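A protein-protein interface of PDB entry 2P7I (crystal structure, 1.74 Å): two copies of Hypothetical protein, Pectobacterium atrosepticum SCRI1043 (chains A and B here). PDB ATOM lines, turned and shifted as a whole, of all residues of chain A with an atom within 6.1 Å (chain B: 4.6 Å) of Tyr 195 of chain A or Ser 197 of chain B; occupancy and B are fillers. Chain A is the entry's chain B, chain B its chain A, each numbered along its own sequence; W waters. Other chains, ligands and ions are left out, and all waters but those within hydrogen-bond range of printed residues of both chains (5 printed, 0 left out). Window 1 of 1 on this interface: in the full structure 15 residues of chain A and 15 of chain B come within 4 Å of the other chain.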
ATOM      1  N   PHE A  40     -17.703 -23.510   6.301  1.00  0.00           N
ATOM      2  CA  PHE A  40     -18.403 -24.676   6.819  1.00  0.00           C
ATOM      3  C   PHE A  40     -18.399 -25.888   5.909  1.00  0.00           C
ATOM      4  O   PHE A  40     -18.798 -26.977   6.352  1.00  0.00           O
ATOM      5  CB  PHE A  40     -19.872 -24.330   7.089  1.00  0.00           C
ATOM      6  CG  PHE A  40     -20.070 -23.200   8.055  1.00  0.00           C
ATOM      7  CD1 PHE A  40     -19.648 -23.338   9.365  1.00  0.00           C
ATOM      8  CD2 PHE A  40     -20.708 -22.013   7.669  1.00  0.00           C
ATOM      9  CE1 PHE A  40     -19.853 -22.325  10.295  1.00  0.00           C
ATOM     10  CE2 PHE A  40     -20.914 -21.000   8.577  1.00  0.00           C
ATOM     11  CZ  PHE A  40     -20.492 -21.148   9.890  1.00  0.00           C
ATOM     12  N   VAL A 193     -29.630 -28.029  14.523  1.00  0.00           N
ATOM     13  CA  VAL A 193     -29.219 -26.722  14.032  1.00  0.00           C
ATOM     14  C   VAL A 193     -27.954 -26.375  14.760  1.00  0.00           C
ATOM     15  O   VAL A 193     -27.945 -26.260  15.988  1.00  0.00           O
ATOM     16  CB  VAL A 193     -30.325 -25.657  14.235  1.00  0.00           C
ATOM     17  CG1 VAL A 193     -29.773 -24.272  13.910  1.00  0.00           C
ATOM     18  CG2 VAL A 193     -31.542 -26.002  13.409  1.00  0.00           C
ATOM     19  N   THR A 194     -26.874 -26.197  14.008  1.00  0.00           N
ATOM     20  CA  THR A 194     -25.541 -26.006  14.531  1.00  0.00           C
ATOM     21  C   THR A 194     -25.121 -24.539  14.563  1.00  0.00           C
ATOM     22  O   THR A 194     -24.394 -24.120  15.451  1.00  0.00           O
ATOM     23  CB  THR A 194     -24.575 -26.781  13.633  1.00  0.00           C
ATOM     24  OG1 THR A 194     -24.952 -28.173  13.642  1.00  0.00           O
ATOM     25  CG2 THR A 194     -23.150 -26.624  14.083  1.00  0.00           C
ATOM     26  N   TYR A 195     -25.556 -23.788  13.543  1.00  0.00           N
ATOM     27  CA  TYR A 195     -25.210 -22.366  13.449  1.00  0.00           C
ATOM     28  C   TYR A 195     -26.342 -21.583  12.843  1.00  0.00           C
ATOM     29  O   TYR A 195     -27.017 -22.044  11.929  1.00  0.00           O
ATOM     30  CB  TYR A 195     -23.914 -22.114  12.674  1.00  0.00           C
ATOM     31  CG  TYR A 195     -22.863 -21.494  13.557  1.00  0.00           C
ATOM     32  CD1 TYR A 195     -22.634 -20.121  13.575  1.00  0.00           C
ATOM     33  CD2 TYR A 195     -22.134 -22.284  14.427  1.00  0.00           C
ATOM     34  CE1 TYR A 195     -21.656 -19.569  14.444  1.00  0.00           C
ATOM     35  CE2 TYR A 195     -21.181 -21.745  15.280  1.00  0.00           C
ATOM     36  CZ  TYR A 195     -20.946 -20.410  15.290  1.00  0.00           C
ATOM     37  OH  TYR A 195     -19.969 -19.958  16.174  1.00  0.00           O
ATOM     38  N   ARG A 196     -26.558 -20.385  13.368  1.00  0.00           N
ATOM     39  CA  ARG A 196     -27.545 -19.455  12.847  1.00  0.00           C
ATOM     40  C   ARG A 196     -26.797 -18.175  12.480  1.00  0.00           C
ATOM     41  O   ARG A 196     -25.958 -17.703  13.261  1.00  0.00           O
ATOM     42  CB  ARG A 196     -28.587 -19.082  13.889  1.00  0.00           C
ATOM     43  CG  ARG A 196     -29.212 -20.276  14.603  1.00  0.00           C
ATOM     44  CD  ARG A 196     -29.325 -20.146  16.068  1.00  0.00           C
ATOM     45  NE  ARG A 196     -29.884 -21.385  16.582  1.00  0.00           N
ATOM     46  CZ  ARG A 196     -29.150 -22.442  16.932  1.00  0.00           C
ATOM     47  NH1 ARG A 196     -27.824 -22.366  16.965  1.00  0.00           N
ATOM     48  NH2 ARG A 196     -29.734 -23.566  17.340  1.00  0.00           N
ATOM     49  N   SER A 197     -27.085 -17.654  11.298  1.00  0.00           N
ATOM     50  CA  SER A 197     -26.471 -16.399  10.843  1.00  0.00           C
ATOM     51  C   SER A 197     -27.355 -15.746   9.794  1.00  0.00           C
ATOM     52  O   SER A 197     -28.456 -16.204   9.506  1.00  0.00           O
ATOM     53  CB  SER A 197     -25.056 -16.640  10.280  1.00  0.00           C
ATOM     54  OG  SER A 197     -24.301 -15.414  10.210  1.00  0.00           O
ATOM     55  N   GLN A 231     -23.523 -10.125   9.448  1.00  0.00           N
ATOM     56  CA  GLN A 231     -23.215 -11.187  10.408  1.00  0.00           C
ATOM     57  C   GLN A 231     -23.469 -10.782  11.852  1.00  0.00           C
ATOM     58  O   GLN A 231     -23.759 -11.645  12.686  1.00  0.00           O
ATOM     59  CB  GLN A 231     -21.777 -11.667  10.251  1.00  0.00           C
ATOM     60  CG  GLN A 231     -21.569 -12.364   8.919  1.00  0.00           C
ATOM     61  CD  GLN A 231     -20.160 -12.865   8.716  1.00  0.00           C
ATOM     62  OE1 GLN A 231     -19.265 -12.513   9.470  1.00  0.00           O
ATOM     63  NE2 GLN A 231     -19.952 -13.642   7.638  1.00  0.00           N
ATOM     64  N   PHE A 241     -29.733 -17.927   7.426  1.00  0.00           N
ATOM     65  CA  PHE A 241     -28.884 -19.058   7.108  1.00  0.00           C
ATOM     66  C   PHE A 241     -28.775 -19.891   8.359  1.00  0.00           C
ATOM     67  O   PHE A 241     -28.273 -19.437   9.403  1.00  0.00           O
ATOM     68  CB  PHE A 241     -27.508 -18.526   6.612  1.00  0.00           C
ATOM     69  CG  PHE A 241     -26.397 -19.553   6.517  1.00  0.00           C
ATOM     70  CD1 PHE A 241     -26.638 -20.889   6.188  1.00  0.00           C
ATOM     71  CD2 PHE A 241     -25.085 -19.159   6.711  1.00  0.00           C
ATOM     72  CE1 PHE A 241     -25.581 -21.807   6.138  1.00  0.00           C
ATOM     73  CE2 PHE A 241     -24.030 -20.071   6.612  1.00  0.00           C
ATOM     74  CZ  PHE A 241     -24.278 -21.400   6.373  1.00  0.00           C
ATOM     75  N   LEU A 242     -29.313 -21.098   8.274  1.00  0.00           N
ATOM     76  CA  LEU A 242     -29.070 -22.129   9.242  1.00  0.00           C
ATOM     77  C   LEU A 242     -28.116 -23.225   8.716  1.00  0.00           C
ATOM     78  O   LEU A 242     -28.344 -23.808   7.678  1.00  0.00           O
ATOM     79  CB  LEU A 242     -30.383 -22.791   9.696  1.00  0.00           C
ATOM     80  CG  LEU A 242     -31.483 -21.939  10.359  1.00  0.00           C
ATOM     81  CD1 LEU A 242     -32.579 -22.971  10.873  1.00  0.00           C
ATOM     82  CD2 LEU A 242     -30.952 -21.137  11.491  1.00  0.00           C
ATOM     83  N   LEU A 243     -27.067 -23.496   9.473  1.00  0.00           N
ATOM     84  CA  LEU A 243     -26.190 -24.641   9.230  1.00  0.00           C
ATOM     85  C   LEU A 243     -26.691 -25.761  10.076  1.00  0.00           C
ATOM     86  O   LEU A 243     -26.776 -25.660  11.310  1.00  0.00           O
ATOM     87  CB  LEU A 243     -24.735 -24.350   9.626  1.00  0.00           C
ATOM     88  CG  LEU A 243     -23.726 -25.451   9.216  1.00  0.00           C
ATOM     89  CD1 LEU A 243     -23.537 -25.431   7.665  1.00  0.00           C
ATOM     90  CD2 LEU A 243     -22.407 -25.228   9.940  1.00  0.00           C
ATOM     91  N   CYS A 244     -27.028 -26.867   9.449  1.00  0.00           N
ATOM     92  CA  CYS A 244     -27.633 -27.986  10.143  1.00  0.00           C
ATOM     93  C   CYS A 244     -26.851 -29.272   9.914  1.00  0.00           C
ATOM     94  O   CYS A 244     -26.173 -29.437   8.888  1.00  0.00           O
ATOM     95  CB  CYS A 244     -29.035 -28.218   9.591  1.00  0.00           C
ATOM     96  SG  CYS A 244     -30.175 -26.809   9.767  1.00  0.00           S
ATOM     97  N   ALA B  36     -19.320 -23.405  19.838  1.00  0.00           N
ATOM     98  CA  ALA B  36     -19.221 -22.365  18.817  1.00  0.00           C
ATOM     99  C   ALA B  36     -18.079 -22.586  17.839  1.00  0.00           C
ATOM    100  O   ALA B  36     -18.150 -22.193  16.688  1.00  0.00           O
ATOM    101  CB  ALA B  36     -19.079 -21.000  19.505  1.00  0.00           C
ATOM    102  N   PRO B  39     -17.974 -26.191  14.463  1.00  0.00           N
ATOM    103  CA  PRO B  39     -18.172 -26.221  12.997  1.00  0.00           C
ATOM    104  C   PRO B  39     -17.084 -25.525  12.163  1.00  0.00           C
ATOM    105  O   PRO B  39     -17.019 -25.707  10.954  1.00  0.00           O
ATOM    106  CB  PRO B  39     -19.529 -25.557  12.806  1.00  0.00           C
ATOM    107  CG  PRO B  39     -19.874 -24.925  14.045  1.00  0.00           C
ATOM    108  CD  PRO B  39     -19.034 -25.430  15.144  1.00  0.00           C
ATOM    109  N   PHE B  40     -16.211 -24.788  12.801  1.00  0.00           N
ATOM    110  CA  PHE B  40     -15.138 -24.086  12.095  1.00  0.00           C
ATOM    111  C   PHE B  40     -13.783 -24.807  12.179  1.00  0.00           C
ATOM    112  O   PHE B  40     -12.844 -24.454  11.441  1.00  0.00           O
ATOM    113  CB  PHE B  40     -14.966 -22.713  12.713  1.00  0.00           C
ATOM    114  CG  PHE B  40     -16.102 -21.781  12.494  1.00  0.00           C
ATOM    115  CD1 PHE B  40     -16.325 -21.235  11.229  1.00  0.00           C
ATOM    116  CD2 PHE B  40     -16.916 -21.389  13.551  1.00  0.00           C
ATOM    117  CE1 PHE B  40     -17.335 -20.324  11.023  1.00  0.00           C
ATOM    118  CE2 PHE B  40     -17.932 -20.457  13.351  1.00  0.00           C
ATOM    119  CZ  PHE B  40     -18.159 -19.947  12.078  1.00  0.00           C
ATOM    120  N   LEU B 179     -17.383  -5.809  19.080  1.00  0.00           N
ATOM    121  CA  LEU B 179     -17.145  -6.227  17.668  1.00  0.00           C
ATOM    122  C   LEU B 179     -16.386  -5.193  16.815  1.00  0.00           C
ATOM    123  O   LEU B 179     -15.543  -5.573  15.976  1.00  0.00           O
ATOM    124  CB  LEU B 179     -18.452  -6.623  17.007  1.00  0.00           C
ATOM    125  CG  LEU B 179     -18.995  -7.993  17.484  1.00  0.00           C
ATOM    126  CD1 LEU B 179     -20.468  -8.122  17.223  1.00  0.00           C
ATOM    127  CD2 LEU B 179     -18.236  -9.137  16.799  1.00  0.00           C
ATOM    128  N   TYR B 195     -15.562 -14.617   9.898  1.00  0.00           N
ATOM    129  CA  TYR B 195     -16.888 -14.708  10.533  1.00  0.00           C
ATOM    130  C   TYR B 195     -16.896 -13.951  11.849  1.00  0.00           C
ATOM    131  O   TYR B 195     -15.897 -13.913  12.561  1.00  0.00           O
ATOM    132  CB  TYR B 195     -17.305 -16.144  10.806  1.00  0.00           C
ATOM    133  CG  TYR B 195     -18.457 -16.575   9.956  1.00  0.00           C
ATOM    134  CD1 TYR B 195     -19.778 -16.388  10.374  1.00  0.00           C
ATOM    135  CD2 TYR B 195     -18.235 -17.089   8.709  1.00  0.00           C
ATOM    136  CE1 TYR B 195     -20.846 -16.759   9.545  1.00  0.00           C
ATOM    137  CE2 TYR B 195     -19.281 -17.467   7.882  1.00  0.00           C
ATOM    138  CZ  TYR B 195     -20.573 -17.300   8.305  1.00  0.00           C
ATOM    139  OH  TYR B 195     -21.585 -17.677   7.445  1.00  0.00           O
ATOM    140  N   ARG B 196     -18.020 -13.295  12.114  1.00  0.00           N
ATOM    141  CA  ARG B 196     -18.241 -12.561  13.361  1.00  0.00           C
ATOM    142  C   ARG B 196     -19.460 -13.171  14.028  1.00  0.00           C
ATOM    143  O   ARG B 196     -20.470 -13.437  13.373  1.00  0.00           O
ATOM    144  CB  ARG B 196     -18.555 -11.108  13.084  1.00  0.00           C
ATOM    145  CG  ARG B 196     -17.543 -10.452  12.156  1.00  0.00           C
ATOM    146  CD  ARG B 196     -18.190  -9.632  11.074  1.00  0.00           C
ATOM    147  NE  ARG B 196     -17.104  -9.107  10.245  1.00  0.00           N
ATOM    148  CZ  ARG B 196     -16.570  -9.739   9.211  1.00  0.00           C
ATOM    149  NH1 ARG B 196     -17.097 -10.853   8.729  1.00  0.00           N
ATOM    150  NH2 ARG B 196     -15.553  -9.200   8.588  1.00  0.00           N
ATOM    151  N   SER B 197     -19.328 -13.474  15.310  1.00  0.00           N
ATOM    152  CA  SER B 197     -20.444 -14.038  16.062  1.00  0.00           C
ATOM    153  C   SER B 197     -20.333 -13.719  17.532  1.00  0.00           C
ATOM    154  O   SER B 197     -19.436 -12.982  17.936  1.00  0.00           O
ATOM    155  CB  SER B 197     -20.535 -15.552  15.860  1.00  0.00           C
ATOM    156  OG  SER B 197     -21.801 -16.028  16.293  1.00  0.00           O
ATOM    157  N   GLY B 198     -21.323 -14.203  18.283  1.00  0.00           N
ATOM    158  CA  GLY B 198     -21.377 -14.090  19.756  1.00  0.00           C
ATOM    159  C   GLY B 198     -21.681 -15.387  20.446  1.00  0.00           C
ATOM    160  O   GLY B 198     -22.271 -16.257  19.871  1.00  0.00           O
ATOM    161  N   TYR B 227     -27.627 -19.760  24.398  1.00  0.00           N
ATOM    162  CA  TYR B 227     -26.570 -19.928  23.396  1.00  0.00           C
ATOM    163  C   TYR B 227     -27.184 -19.821  22.015  1.00  0.00           C
ATOM    164  O   TYR B 227     -26.661 -19.112  21.177  1.00  0.00           O
ATOM    165  CB  TYR B 227     -25.871 -21.269  23.566  1.00  0.00           C
ATOM    166  CG  TYR B 227     -24.941 -21.632  22.403  1.00  0.00           C
ATOM    167  CD1 TYR B 227     -23.676 -21.071  22.290  1.00  0.00           C
ATOM    168  CD2 TYR B 227     -25.325 -22.548  21.468  1.00  0.00           C
ATOM    169  CE1 TYR B 227     -22.853 -21.420  21.255  1.00  0.00           C
ATOM    170  CE2 TYR B 227     -24.498 -22.907  20.407  1.00  0.00           C
ATOM    171  CZ  TYR B 227     -23.284 -22.338  20.298  1.00  0.00           C
ATOM    172  OH  TYR B 227     -22.464 -22.705  19.244  1.00  0.00           O
ATOM    173  N   GLN B 231     -26.522 -16.309  19.065  1.00  0.00           N
ATOM    174  CA  GLN B 231     -26.015 -16.317  17.720  1.00  0.00           C
ATOM    175  C   GLN B 231     -26.791 -15.353  16.846  1.00  0.00           C
ATOM    176  O   GLN B 231     -26.261 -14.857  15.827  1.00  0.00           O
ATOM    177  CB  GLN B 231     -26.142 -17.726  17.139  1.00  0.00           C
ATOM    178  CG  GLN B 231     -25.129 -18.672  17.789  1.00  0.00           C
ATOM    179  CD  GLN B 231     -24.962 -19.972  17.051  1.00  0.00           C
ATOM    180  OE1 GLN B 231     -25.832 -20.390  16.288  1.00  0.00           O
ATOM    181  NE2 GLN B 231     -23.839 -20.634  17.294  1.00  0.00           N
ATOM    182  N   PRO B 234     -25.261 -11.279  18.063  1.00  0.00           N
ATOM    183  CA  PRO B 234     -23.888 -11.307  18.493  1.00  0.00           C
ATOM    184  C   PRO B 234     -23.479 -10.134  19.350  1.00  0.00           C
ATOM    185  O   PRO B 234     -22.685 -10.298  20.243  1.00  0.00           O
ATOM    186  CB  PRO B 234     -23.124 -11.266  17.149  1.00  0.00           C
ATOM    187  CG  PRO B 234     -23.971 -11.977  16.249  1.00  0.00           C
ATOM    188  CD  PRO B 234     -25.370 -11.554  16.609  1.00  0.00           C
ATOM    189  N   ILE B 240     -17.704 -12.155  22.433  1.00  0.00           N
ATOM    190  CA  ILE B 240     -17.728 -12.030  20.997  1.00  0.00           C
ATOM    191  C   ILE B 240     -16.606 -12.861  20.397  1.00  0.00           C
ATOM    192  O   ILE B 240     -15.565 -13.067  21.022  1.00  0.00           O
ATOM    193  CB  ILE B 240     -17.578 -10.552  20.546  1.00  0.00           C
ATOM    194  CG1 ILE B 240     -16.544  -9.786  21.373  1.00  0.00           C
ATOM    195  CG2 ILE B 240     -18.979  -9.839  20.724  1.00  0.00           C
ATOM    196  CD1 ILE B 240     -16.273  -8.397  20.771  1.00  0.00           C
ATOM    197  N   PHE B 241     -16.852 -13.336  19.177  1.00  0.00           N
ATOM    198  CA  PHE B 241     -16.027 -14.329  18.537  1.00  0.00           C
ATOM    199  C   PHE B 241     -15.765 -13.954  17.094  1.00  0.00           C
ATOM    200  O   PHE B 241     -16.711 -13.781  16.332  1.00  0.00           O
ATOM    201  CB  PHE B 241     -16.777 -15.657  18.694  1.00  0.00           C
ATOM    202  CG  PHE B 241     -16.299 -16.787  17.812  1.00  0.00           C
ATOM    203  CD1 PHE B 241     -14.972 -16.958  17.488  1.00  0.00           C
ATOM    204  CD2 PHE B 241     -17.213 -17.785  17.421  1.00  0.00           C
ATOM    205  CE1 PHE B 241     -14.561 -18.004  16.665  1.00  0.00           C
ATOM    206  CE2 PHE B 241     -16.816 -18.809  16.604  1.00  0.00           C
ATOM    207  CZ  PHE B 241     -15.478 -18.927  16.233  1.00  0.00           C
HETATM  208  O   HOH W   1     -24.075 -15.870  14.554  1.00  0.00           O
HETATM  209  O   HOH W   2     -21.540 -18.613  18.296  1.00  0.00           O
HETATM  210  O   HOH W   3     -23.628 -24.909  17.812  1.00  0.00           O
HETATM  211  O   HOH W   4     -23.237 -14.371  12.387  1.00  0.00           O
HETATM  212  O   HOH W   5     -23.090 -15.225   7.182  1.00  0.00           O
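O of Ala 36 of chain B lies within hydrogen-bond range of OH of Tyr 195 of chain A, 2.9 Å away. OE1 of Gln 231 of chain A is in hydrogen-bond range of NH1 of Arg 196 of chain B (2.8 Å). The side-chain amide oxygen (OE1) of Gln 231 of chain B lies within hydrogen-bond range of the guanidinium group (NH1) of Arg 196 of chain A, at 2.9 Å.
Of the 13 printed residues of chain B, 9 touch a printed residue of chain A. Printed residues of chain B that touch a printed residue of chain A: Ala 36, Pro 39, Phe 40, Tyr 195, Arg 196, Ser 197, Gln 231, Pro 234 and Phe 241. Hydrophobic or aromatic side chains of chain A that line the printed part of chain B: Phe 40, Tyr 195 and Phe 241.
Printed residues of chain B within 4 Å of Tyr 195 of chain A: Ala 36 (2.9 Å), Pro 39 (3.5 Å), Phe 40 (3.5 Å), Ser 197 (3.997 Å), Gln 231 (3.5 Å) and Phe 241 (3.4 Å). Of the printed residues of chain B, Arg 196 of chain A touches Gln 231. Leu 179 of chain B touches none of the printed residues of chain A. Of the printed residues of chain A, Tyr 195 of chain B touches Phe 40 (3.6 Å), Ser 197 (3.8 Å), Gln 231 (3.4 Å) and Phe 241 (3.5 Å). Of the printed residues of chain A, Ser 197 of chain B touches Tyr 195 (3.997 Å). Of the printed residues of chain A, Gln 231 of chain B touches Thr 194 (3.98 Å), Tyr 195 (3.5 Å) and Arg 196 (2.9 Å).
Water W3 lies within hydrogen-bond range of the backbone carbonyl oxygen (O) of Thr 194 of chain A (2.6 Å) and the side-chain hydroxyl (OH) of Tyr 227 of chain B (2.9 Å). Water W4 lies within hydrogen-bond range of the side-chain hydroxyl of Ser 197 of chain A, the backbone carbonyl oxygen of Gln 231 of chain A and the backbone carbonyl oxygen of Arg 196 of chain B. Water W1 lies within hydrogen-bond range of O of Gln 231 of chain B, OG of Ser 197 of chain B and O of Arg 196 of chain A. Water W5 lies within hydrogen-bond range of OH of Tyr 195 of chain B (2.9 Å) and OG of Ser 197 of chain A (3.3 Å). Water W2 lies within hydrogen-bond range of the backbone carbonyl oxygen (O) of Gly 198 of chain B, the side-chain hydroxyl (OH) of Tyr 195 of chain A, the side-chain amide nitrogen (NE2) of Gln 231 of chain B and the side-chain hydroxyl (OG) of Ser 197 of chain B.
Among the printed residues, pairs that only touch across the chains: Phe 40 of chain A with Pro 39 of chain B, Phe 40 of chain A with Phe 40 of chain B, Phe 40 of chain A with Tyr 195 of chain B, Thr 194 of chain A with Pro 39 of chain B, Thr 194 of chain A with Gln 231 of chain B, Tyr 195 of chain A with Pro 39 of chain B, Tyr 195 of chain A with Phe 40 of chain B, Tyr 195 of chain A with Ser 197 of chain B, Tyr 195 of chain A with Gln 231 of chain B, Tyr 195 of chain A with Phe 241 of chain B, Ser 197 of chain A with Tyr 195 of chain B, Gln 231 of chain A with Tyr 195 of chain B, Gln 231 of chain A with Pro 234 of chain B and Phe 241 of chain A with Tyr 195 of chain B.
Phe 40 of chain B touches its own counterpart, Phe 40 of chain A. Phe 40 of chain A touches Tyr 195 of chain B, and with the chains exchanged Tyr 195 of chain A touches Phe 40 of chain B. Tyr 195 of chain A touches Ser 197 of chain B, and with the chains exchanged Ser 197 of chain A touches Tyr 195 of chain B. Tyr 195 of chain A touches Gln 231 of chain B, and with the chains exchanged Gln 231 of chain A touches Tyr 195 of chain B. Of the 17 pairs that touch across the chains among the printed residues, 11 have their exchanged pair printed and touching as well.
The backbone NH (N) of Ala 36 of chain B sits at hydrogen-bond distance from the side-chain hydroxyl (OH) of Tyr 227 of chain B. N of Ser 197 of chain B is in hydrogen-bond range of O of Phe 241 of chain B, at 2.8 Å. NE2 of Gln 231 of chain B lies within hydrogen-bond range of OH of Tyr 227 of chain B (3.2 Å). The backbone NH of Thr 194 of chain A sits at hydrogen-bond distance from the backbone carbonyl oxygen of Leu 243 of chain A, at 2.8 Å. The backbone carbonyl oxygen of Tyr 195 of chain A is in hydrogen-bond range of the backbone NH of Leu 243 of chain A (2.9 Å). O of Phe 241 of chain A is in hydrogen-bond range of N of Ser 197 of chain A, at 2.9 Å.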
